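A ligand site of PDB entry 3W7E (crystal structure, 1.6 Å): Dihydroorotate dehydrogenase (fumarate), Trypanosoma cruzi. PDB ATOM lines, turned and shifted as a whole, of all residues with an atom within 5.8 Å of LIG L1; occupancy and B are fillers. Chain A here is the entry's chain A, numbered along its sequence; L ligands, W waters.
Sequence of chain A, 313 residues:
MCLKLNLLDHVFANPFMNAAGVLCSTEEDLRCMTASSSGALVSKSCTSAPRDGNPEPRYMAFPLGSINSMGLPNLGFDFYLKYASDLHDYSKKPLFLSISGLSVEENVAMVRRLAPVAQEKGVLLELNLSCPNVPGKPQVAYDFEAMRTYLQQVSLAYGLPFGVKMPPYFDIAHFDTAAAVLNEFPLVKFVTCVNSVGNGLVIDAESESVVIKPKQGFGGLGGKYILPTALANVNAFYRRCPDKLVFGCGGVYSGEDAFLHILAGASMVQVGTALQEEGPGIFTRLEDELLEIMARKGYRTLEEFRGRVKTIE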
ATOM      1  N   LYS A  44      10.484 -36.154  16.728  1.00  0.00           N
ATOM      2  CA  LYS A  44      10.813 -35.062  17.608  1.00  0.00           C
ATOM      3  C   LYS A  44      11.201 -33.825  16.812  1.00  0.00           C
ATOM      4  O   LYS A  44      12.018 -33.935  15.924  1.00  0.00           O
ATOM      5  CB  LYS A  44      11.994 -35.492  18.428  1.00  0.00           C
ATOM      6  CG  LYS A  44      12.556 -34.426  19.327  1.00  0.00           C
ATOM      7  CD  LYS A  44      11.719 -33.829  20.482  1.00  0.00           C
ATOM      8  CE  LYS A  44      12.167 -32.491  21.075  1.00  0.00           C
ATOM      9  NZ  LYS A  44      11.284 -31.961  22.275  1.00  0.00           N
ATOM     10  N   SER A  45      10.653 -32.663  17.168  1.00  0.00           N
ATOM     11  CA  SER A  45      11.011 -31.367  16.505  1.00  0.00           C
ATOM     12  C   SER A  45      12.540 -31.267  16.584  1.00  0.00           C
ATOM     13  O   SER A  45      13.115 -31.452  17.649  1.00  0.00           O
ATOM     14  CB  SER A  45      10.447 -30.158  17.220  1.00  0.00           C
ATOM     15  OG  SER A  45       9.041 -30.153  17.086  1.00  0.00           O
ATOM     16  N   THR A  47      16.447 -29.458  15.294  1.00  0.00           N
ATOM     17  CA  THR A  47      17.331 -28.348  14.864  1.00  0.00           C
ATOM     18  C   THR A  47      18.384 -28.959  13.931  1.00  0.00           C
ATOM     19  O   THR A  47      18.563 -30.161  13.882  1.00  0.00           O
ATOM     20  CB  THR A  47      17.980 -27.682  16.122  1.00  0.00           C
ATOM     21  OG1 THR A  47      18.457 -28.691  17.004  1.00  0.00           O
ATOM     22  CG2 THR A  47      17.025 -26.797  16.800  1.00  0.00           C
ATOM     23  N   ARG A  51      21.049 -31.365  20.051  1.00  0.00           N
ATOM     24  CA  ARG A  51      20.960 -30.634  21.292  1.00  0.00           C
ATOM     25  C   ARG A  51      20.797 -31.620  22.401  1.00  0.00           C
ATOM     26  O   ARG A  51      20.025 -32.576  22.318  1.00  0.00           O
ATOM     27  CB  ARG A  51      19.714 -29.711  21.348  1.00  0.00           C
ATOM     28  CG  ARG A  51      19.762 -28.584  20.314  1.00  0.00           C
ATOM     29  CD  ARG A  51      18.475 -27.795  20.313  1.00  0.00           C
ATOM     30  NE  ARG A  51      18.113 -27.235  21.611  1.00  0.00           N
ATOM     31  CZ  ARG A  51      18.497 -26.080  22.074  1.00  0.00           C
ATOM     32  NH1 ARG A  51      19.285 -25.285  21.305  1.00  0.00           N
ATOM     33  NH2 ARG A  51      18.084 -25.698  23.237  1.00  0.00           N
ATOM     34  N   ASN A  54      17.694 -29.072  28.107  1.00  0.00           N
ATOM     35  CA  ASN A  54      17.880 -28.451  29.433  1.00  0.00           C
ATOM     36  C   ASN A  54      18.247 -29.436  30.525  1.00  0.00           C
ATOM     37  O   ASN A  54      18.127 -30.625  30.417  1.00  0.00           O
ATOM     38  CB  ASN A  54      16.581 -27.755  29.825  1.00  0.00           C
ATOM     39  CG  ASN A  54      16.369 -26.459  29.160  1.00  0.00           C
ATOM     40  OD1 ASN A  54      17.323 -25.850  28.627  1.00  0.00           O
ATOM     41  ND2 ASN A  54      15.119 -26.052  29.027  1.00  0.00           N
ATOM     42  N   ASN A  68       6.626 -29.331  31.272  1.00  0.00           N
ATOM     43  CA  ASN A  68       7.925 -29.610  30.753  1.00  0.00           C
ATOM     44  C   ASN A  68       8.620 -28.340  30.326  1.00  0.00           C
ATOM     45  O   ASN A  68       8.043 -27.418  29.777  1.00  0.00           O
ATOM     46  CB  ASN A  68       7.896 -30.612  29.604  1.00  0.00           C
ATOM     47  CG  ASN A  68       7.633 -29.993  28.232  1.00  0.00           C
ATOM     48  OD1 ASN A  68       8.568 -29.532  27.531  1.00  0.00           O
ATOM     49  ND2 ASN A  68       6.385 -30.009  27.785  1.00  0.00           N
ATOM     50  N   SER A  69       9.920 -28.355  30.422  1.00  0.00           N
ATOM     51  CA  SER A  69      10.787 -27.399  29.758  1.00  0.00           C
ATOM     52  C   SER A  69      11.982 -28.180  29.208  1.00  0.00           C
ATOM     53  O   SER A  69      13.103 -28.086  29.743  1.00  0.00           O
ATOM     54  CB  SER A  69      11.254 -26.257  30.719  1.00  0.00           C
ATOM     55  OG  SER A  69      12.053 -25.366  29.950  1.00  0.00           O
ATOM     56  N   MET A  70      11.742 -29.025  28.241  1.00  0.00           N
ATOM     57  CA  MET A  70      12.760 -29.938  27.791  1.00  0.00           C
ATOM     58  C   MET A  70      13.947 -29.247  27.190  1.00  0.00           C
ATOM     59  O   MET A  70      15.042 -29.801  27.314  1.00  0.00           O
ATOM     60  CB  MET A  70      12.155 -30.872  26.764  1.00  0.00           C
ATOM     61  CG  MET A  70      11.005 -31.778  27.124  1.00  0.00           C
ATOM     62  SD  MET A  70      11.308 -32.842  28.504  1.00  0.00           S
ATOM     63  CE  MET A  70      12.390 -34.013  27.800  1.00  0.00           C
ATOM     64  N   GLY A  71      13.785 -28.151  26.494  1.00  0.00           N
ATOM     65  CA  GLY A  71      14.867 -27.441  25.803  1.00  0.00           C
ATOM     66  C   GLY A  71      15.202 -27.964  24.430  1.00  0.00           C
ATOM     67  O   GLY A  71      16.350 -27.856  24.022  1.00  0.00           O
ATOM     68  N   LEU A  72      14.262 -28.632  23.819  1.00  0.00           N
ATOM     69  CA  LEU A  72      14.421 -29.229  22.501  1.00  0.00           C
ATOM     70  C   LEU A  72      15.671 -30.179  22.402  1.00  0.00           C
ATOM     71  O   LEU A  72      16.432 -30.152  21.442  1.00  0.00           O
ATOM     72  CB  LEU A  72      14.406 -28.183  21.359  1.00  0.00           C
ATOM     73  CG  LEU A  72      14.009 -28.865  20.028  1.00  0.00           C
ATOM     74  CD1 LEU A  72      12.507 -28.896  19.859  1.00  0.00           C
ATOM     75  CD2 LEU A  72      14.691 -28.204  18.827  1.00  0.00           C
ATOM     76  N   PRO A  73      15.799 -31.120  23.304  1.00  0.00           N
ATOM     77  CA  PRO A  73      16.793 -32.192  23.079  1.00  0.00           C
ATOM     78  C   PRO A  73      16.419 -32.980  21.829  1.00  0.00           C
ATOM     79  O   PRO A  73      15.254 -33.344  21.586  1.00  0.00           O
ATOM     80  CB  PRO A  73      16.699 -33.045  24.322  1.00  0.00           C
ATOM     81  CG  PRO A  73      15.335 -32.862  24.847  1.00  0.00           C
ATOM     82  CD  PRO A  73      14.813 -31.554  24.311  1.00  0.00           C
ATOM     83  N   SER A 100      11.944 -27.505  14.060  1.00  0.00           N
ATOM     84  CA  SER A 100      11.813 -26.313  14.865  1.00  0.00           C
ATOM     85  C   SER A 100      13.218 -25.741  14.932  1.00  0.00           C
ATOM     86  O   SER A 100      13.919 -25.840  15.952  1.00  0.00           O
ATOM     87  CB  SER A 100      11.183 -26.641  16.192  1.00  0.00           C
ATOM     88  OG  SER A 100      10.593 -25.426  16.685  1.00  0.00           O
ATOM     89  N   GLY A 101      13.576 -25.008  13.909  1.00  0.00           N
ATOM     90  CA  GLY A 101      14.761 -24.191  13.898  1.00  0.00           C
ATOM     91  C   GLY A 101      14.689 -22.965  14.792  1.00  0.00           C
ATOM     92  O   GLY A 101      13.626 -22.415  15.016  1.00  0.00           O
ATOM     93  N   LEU A 102      15.873 -22.439  15.126  1.00  0.00           N
ATOM     94  CA  LEU A 102      16.010 -21.313  16.025  1.00  0.00           C
ATOM     95  C   LEU A 102      16.031 -19.965  15.285  1.00  0.00           C
ATOM     96  O   LEU A 102      16.173 -18.904  15.907  1.00  0.00           O
ATOM     97  CB  LEU A 102      17.267 -21.513  16.899  1.00  0.00           C
ATOM     98  CG  LEU A 102      17.046 -22.646  17.961  1.00  0.00           C
ATOM     99  CD1 LEU A 102      18.389 -22.905  18.636  1.00  0.00           C
ATOM    100  CD2 LEU A 102      16.046 -22.152  18.954  1.00  0.00           C
ATOM    101  N   ASN A 128       7.036 -26.534  13.583  1.00  0.00           N
ATOM    102  CA  ASN A 128       6.679 -26.083  14.908  1.00  0.00           C
ATOM    103  C   ASN A 128       6.943 -24.620  15.023  1.00  0.00           C
ATOM    104  O   ASN A 128       8.106 -24.220  15.165  1.00  0.00           O
ATOM    105  CB  ASN A 128       7.437 -26.956  15.916  1.00  0.00           C
ATOM    106  CG  ASN A 128       7.231 -26.573  17.341  1.00  0.00           C
ATOM    107  OD1 ASN A 128       6.458 -25.777  17.615  1.00  0.00           O
ATOM    108  ND2 ASN A 128       7.967 -27.250  18.215  1.00  0.00           N
ATOM    109  N   SER A 130       6.087 -22.822  17.673  1.00  0.00           N
ATOM    110  CA  SER A 130       6.565 -22.363  19.052  1.00  0.00           C
ATOM    111  C   SER A 130       8.091 -22.209  19.135  1.00  0.00           C
ATOM    112  O   SER A 130       8.633 -22.078  20.231  1.00  0.00           O
ATOM    113  CB  SER A 130       6.013 -23.296  20.055  1.00  0.00           C
ATOM    114  OG  SER A 130       4.520 -23.224  19.976  1.00  0.00           O
ATOM    115  N   CYS A 131       8.858 -22.312  18.052  1.00  0.00           N
ATOM    116  CA  CYS A 131      10.253 -22.075  18.152  1.00  0.00           C
ATOM    117  C   CYS A 131      10.459 -20.640  18.757  1.00  0.00           C
ATOM    118  O   CYS A 131       9.671 -19.744  18.590  1.00  0.00           O
ATOM    119  CB  CYS A 131      10.943 -22.200  16.812  1.00  0.00           C
ATOM    120  SG  CYS A 131      10.013 -21.428  15.444  1.00  0.00           S
ATOM    121  N   PRO A 132      11.513 -20.484  19.545  1.00  0.00           N
ATOM    122  CA  PRO A 132      11.798 -19.173  20.060  1.00  0.00           C
ATOM    123  C   PRO A 132      12.350 -18.389  18.899  1.00  0.00           C
ATOM    124  O   PRO A 132      12.889 -19.010  18.020  1.00  0.00           O
ATOM    125  CB  PRO A 132      12.924 -19.457  21.059  1.00  0.00           C
ATOM    126  CG  PRO A 132      13.696 -20.518  20.346  1.00  0.00           C
ATOM    127  CD  PRO A 132      12.682 -21.361  19.613  1.00  0.00           C
ATOM    128  N   ASN A 195       0.020 -27.013  20.729  1.00  0.00           N
ATOM    129  CA  ASN A 195       1.190 -27.155  21.605  1.00  0.00           C
ATOM    130  C   ASN A 195       0.829 -26.908  23.095  1.00  0.00           C
ATOM    131  O   ASN A 195      -0.339 -26.591  23.399  1.00  0.00           O
ATOM    132  CB  ASN A 195       2.330 -26.236  21.122  1.00  0.00           C
ATOM    133  CG  ASN A 195       3.710 -26.851  21.276  1.00  0.00           C
ATOM    134  OD1 ASN A 195       4.017 -27.426  22.314  1.00  0.00           O
ATOM    135  ND2 ASN A 195       4.521 -26.789  20.207  1.00  0.00           N
ATOM    136  N   SER A 196       1.802 -27.068  23.985  1.00  0.00           N
ATOM    137  CA  SER A 196       1.579 -26.925  25.413  1.00  0.00           C
ATOM    138  C   SER A 196       1.179 -25.502  25.817  1.00  0.00           C
ATOM    139  O   SER A 196       1.688 -24.524  25.271  1.00  0.00           O
ATOM    140  CB  SER A 196       2.814 -27.357  26.203  1.00  0.00           C
ATOM    141  OG  SER A 196       4.004 -26.841  25.622  1.00  0.00           O
ATOM    142  N   LYS A 215      14.167 -22.598  34.059  1.00  0.00           N
ATOM    143  CA  LYS A 215      13.237 -21.473  34.035  1.00  0.00           C
ATOM    144  C   LYS A 215      12.523 -21.266  35.353  1.00  0.00           C
ATOM    145  O   LYS A 215      11.356 -20.898  35.383  1.00  0.00           O
ATOM    146  CB  LYS A 215      12.231 -21.585  32.853  1.00  0.00           C
ATOM    147  CG  LYS A 215      12.833 -21.563  31.499  1.00  0.00           C
ATOM    148  CD  LYS A 215      11.763 -21.822  30.400  1.00  0.00           C
ATOM    149  CE  LYS A 215      10.492 -20.988  30.557  1.00  0.00           C
ATOM    150  NZ  LYS A 215       9.753 -21.108  29.285  1.00  0.00           N
ATOM    151  N   GLY A 220       5.767 -25.677  29.931  1.00  0.00           N
ATOM    152  CA  GLY A 220       4.519 -25.865  29.212  1.00  0.00           C
ATOM    153  C   GLY A 220       3.664 -26.988  29.796  1.00  0.00           C
ATOM    154  O   GLY A 220       4.170 -28.021  30.187  1.00  0.00           O
HETATM  155  O1  LIG L   1      10.771 -27.814  25.563  1.00  0.00           O
HETATM  156  C1  LIG L   1      10.634 -28.344  24.469  1.00  0.00           C
HETATM  157  O2  LIG L   1      11.423 -29.132  23.944  1.00  0.00           O
HETATM  158  C2  LIG L   1       9.247 -28.193  23.910  1.00  0.00           C
HETATM  159  N1  LIG L   1       8.210 -28.649  24.773  1.00  0.00           N
HETATM  160  C3  LIG L   1       6.872 -28.511  24.400  1.00  0.00           C
HETATM  161  O3  LIG L   1       5.963 -28.791  25.167  1.00  0.00           O
HETATM  162  N2  LIG L   1       6.628 -28.008  23.129  1.00  0.00           N
HETATM  163  C4  LIG L   1       7.656 -27.652  22.220  1.00  0.00           C
HETATM  164  O4  LIG L   1       7.309 -27.241  21.097  1.00  0.00           O
HETATM  165  C5  LIG L   1       9.000 -27.690  22.696  1.00  0.00           C
HETATM  166  C6  LIG L   1      10.038 -27.200  21.848  1.00  0.00           C
HETATM  167  C7  LIG L   1       9.988 -25.617  21.692  1.00  0.00           C
HETATM  168  C8  LIG L   1      11.316 -25.231  21.085  1.00  0.00           C
HETATM  169  C9  LIG L   1      12.449 -24.921  21.948  1.00  0.00           C
HETATM  170  C10 LIG L   1      12.290 -24.876  23.318  1.00  0.00           C
HETATM  171  C11 LIG L   1      13.387 -24.591  24.119  1.00  0.00           C
HETATM  172  O5  LIG L   1      13.251 -24.599  25.517  1.00  0.00           O
HETATM  173  C12 LIG L   1      12.049 -24.929  26.307  1.00  0.00           C
HETATM  174  C13 LIG L   1      14.576 -24.316  23.433  1.00  0.00           C
HETATM  175  C14 LIG L   1      14.770 -24.335  22.124  1.00  0.00           C
HETATM  176  C15 LIG L   1      13.687 -24.649  21.304  1.00  0.00           C
HETATM  177  C16 LIG L   1      13.821 -24.646  19.897  1.00  0.00           C
HETATM  178  C17 LIG L   1      12.758 -24.906  19.019  1.00  0.00           C
HETATM  179  C18 LIG L   1      11.524 -25.224  19.689  1.00  0.00           C
HETATM  180  N1  LG2 L   2       5.547 -30.194  20.646  1.00  0.00           N
HETATM  181  C1  LG2 L   2       6.233 -30.013  19.514  1.00  0.00           C
HETATM  182  O1  LG2 L   2       5.600 -29.613  18.519  1.00  0.00           O
HETATM  183  N2  LG2 L   2       7.530 -30.425  19.352  1.00  0.00           N
HETATM  184  C2  LG2 L   2       8.260 -30.977  20.341  1.00  0.00           C
HETATM  185  O2  LG2 L   2       9.434 -31.339  20.226  1.00  0.00           O
HETATM  186  C3  LG2 L   2       7.598 -31.155  21.631  1.00  0.00           C
HETATM  187  N3  LG2 L   2       8.199 -31.771  22.639  1.00  0.00           N
HETATM  188  C4  LG2 L   2       7.528 -32.102  23.740  1.00  0.00           C
HETATM  189  C5  LG2 L   2       8.117 -32.912  24.747  1.00  0.00           C
HETATM  190  C6  LG2 L   2       7.408 -33.290  25.869  1.00  0.00           C
HETATM  191  C7  LG2 L   2       8.170 -34.107  26.949  1.00  0.00           C
HETATM  192  C8  LG2 L   2       6.009 -32.972  25.960  1.00  0.00           C
HETATM  193  C9  LG2 L   2       5.225 -33.377  27.131  1.00  0.00           C
HETATM  194  C10 LG2 L   2       5.393 -32.206  24.983  1.00  0.00           C
HETATM  195  C11 LG2 L   2       6.089 -31.804  23.872  1.00  0.00           C
HETATM  196  N4  LG2 L   2       5.509 -31.065  22.835  1.00  0.00           N
HETATM  197  C12 LG2 L   2       6.178 -30.780  21.680  1.00  0.00           C
HETATM  198  C13 LG2 L   2       4.094 -30.739  22.889  1.00  0.00           C
HETATM  199  C14 LG2 L   2       3.165 -31.858  22.573  1.00  0.00           C
HETATM  200  O3  LG2 L   2       3.395 -32.223  21.192  1.00  0.00           O
HETATM  201  C15 LG2 L   2       1.693 -31.523  22.745  1.00  0.00           C
HETATM  202  O4  LG2 L   2       1.429 -30.415  21.870  1.00  0.00           O
HETATM  203  C16 LG2 L   2       1.378 -31.054  24.182  1.00  0.00           C
HETATM  204  O5  LG2 L   2       2.023 -31.925  25.147  1.00  0.00           O
HETATM  205  C17 LG2 L   2      -0.145 -31.150  24.368  1.00  0.00           C
HETATM  206  O6  LG2 L   2      -0.698 -32.440  24.239  1.00  0.00           O
HETATM  207  P1  LG2 L   2      -1.043 -33.406  25.489  1.00  0.00           P
HETATM  208  O7  LG2 L   2      -1.505 -34.699  24.860  1.00  0.00           O
HETATM  209  O8  LG2 L   2      -2.073 -32.688  26.310  1.00  0.00           O
HETATM  210  O9  LG2 L   2       0.264 -33.571  26.254  1.00  0.00           O
HETATM  211  O   HOH W   1      14.645 -23.258  28.085  1.00  0.00           O
HETATM  212  O   HOH W   2       8.716 -26.113  26.805  1.00  0.00           O
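A nitrogen (N2) of LIG L1 is in hydrogen-bond range of the side-chain amide oxygen (OD1) of Asn 195 (2.8 Å).
The side-chain hydroxyl (OG) of Ser 196 lies within hydrogen-bond range of an oxygen (O3) of LIG L1 (2.8 Å).
O2 of LIG L1 is in hydrogen-bond range of N of Leu 72 (2.9 Å).
OD1 of Asn 68 sits at hydrogen-bond distance from N1 of LIG L1, at 2.9 Å.
ND2 of Asn 128 lies within hydrogen-bond range of O4 of LIG L1 (3.0 Å).
N of Met 70 sits at hydrogen-bond distance from O1 of LIG L1.
The backbone NH (N) of Gly 71 lies within hydrogen-bond range of an oxygen (O1) of LIG L1 (3.2 Å).
NZ of Lys 44 is in salt-bridge range of O2 of LIG L1, at 3.3 Å.
An oxygen (O1) of LG2 L2 lies within hydrogen-bond range of the side-chain amide nitrogen (ND2) of Asn 195.
ND2 of Asn 128 is in hydrogen-bond range of O1 of LG2 L2 (3.4 Å).
An oxygen (O2) of LG2 L2 lies within hydrogen-bond range of the side-chain amino group (NZ) of Lys 44.
OG of Ser 45 is in hydrogen-bond range of N2 of LG2 L2.
N2 of LIG L1 sits close to N1 of LG2 L2.
The side-chain hydroxyl of Ser 196 sits at hydrogen-bond distance from the side-chain amide oxygen of Asn 195 (3.4 Å).
ND2 of Asn 195 sits at hydrogen-bond distance from OD1 of Asn 128 (3.4 Å).
The backbone carbonyl oxygen (O) of Leu 72 sits close to the guanidinium group (NE) of Arg 51 (3.4 Å).
The side-chain hydroxyl of Ser 100 sits at hydrogen-bond distance from the backbone carbonyl oxygen of Asn 128 (3.2 Å).
O of Asn 128 sits at hydrogen-bond distance from SG of Cys 131 (3.4 Å).
The side-chain amide oxygen (OD1) of Asn 128 sits at hydrogen-bond distance from the backbone NH (N) of Ser 130 (3.0 Å).
N of Asn 54 is in hydrogen-bond range of O of Met 70 (2.9 Å).
O of Gly 71 sits at hydrogen-bond distance from NH2 of Arg 51, at 2.9 Å.
Residues that only touch LIG L1: Ser 100, Leu 102, Pro 132, Ser 69, Cys 131 and Arg 51.
Hydrophobic or aromatic side chains that line LIG L1: Met 70, Leu 72, Leu 102 and Pro 132.
14 residues have an atom within 4 Å of LIG L1: Lys 44, Arg 51, Asn 68, Ser 69, Met 70, Gly 71, Leu 72, Ser 100, Leu 102, Asn 128, Cys 131, Pro 132, Asn 195 and Ser 196.
Along chain A the residues within 4 Å of LIG L1 span positions 44 to 196.
Water W2 bridges O1 of LIG L1 and O of Asn 68.
Water W1 bridges the side-chain amide nitrogen of Asn 54 (3.0 Å) and an oxygen (O5) of LIG L1 (3.2 Å).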
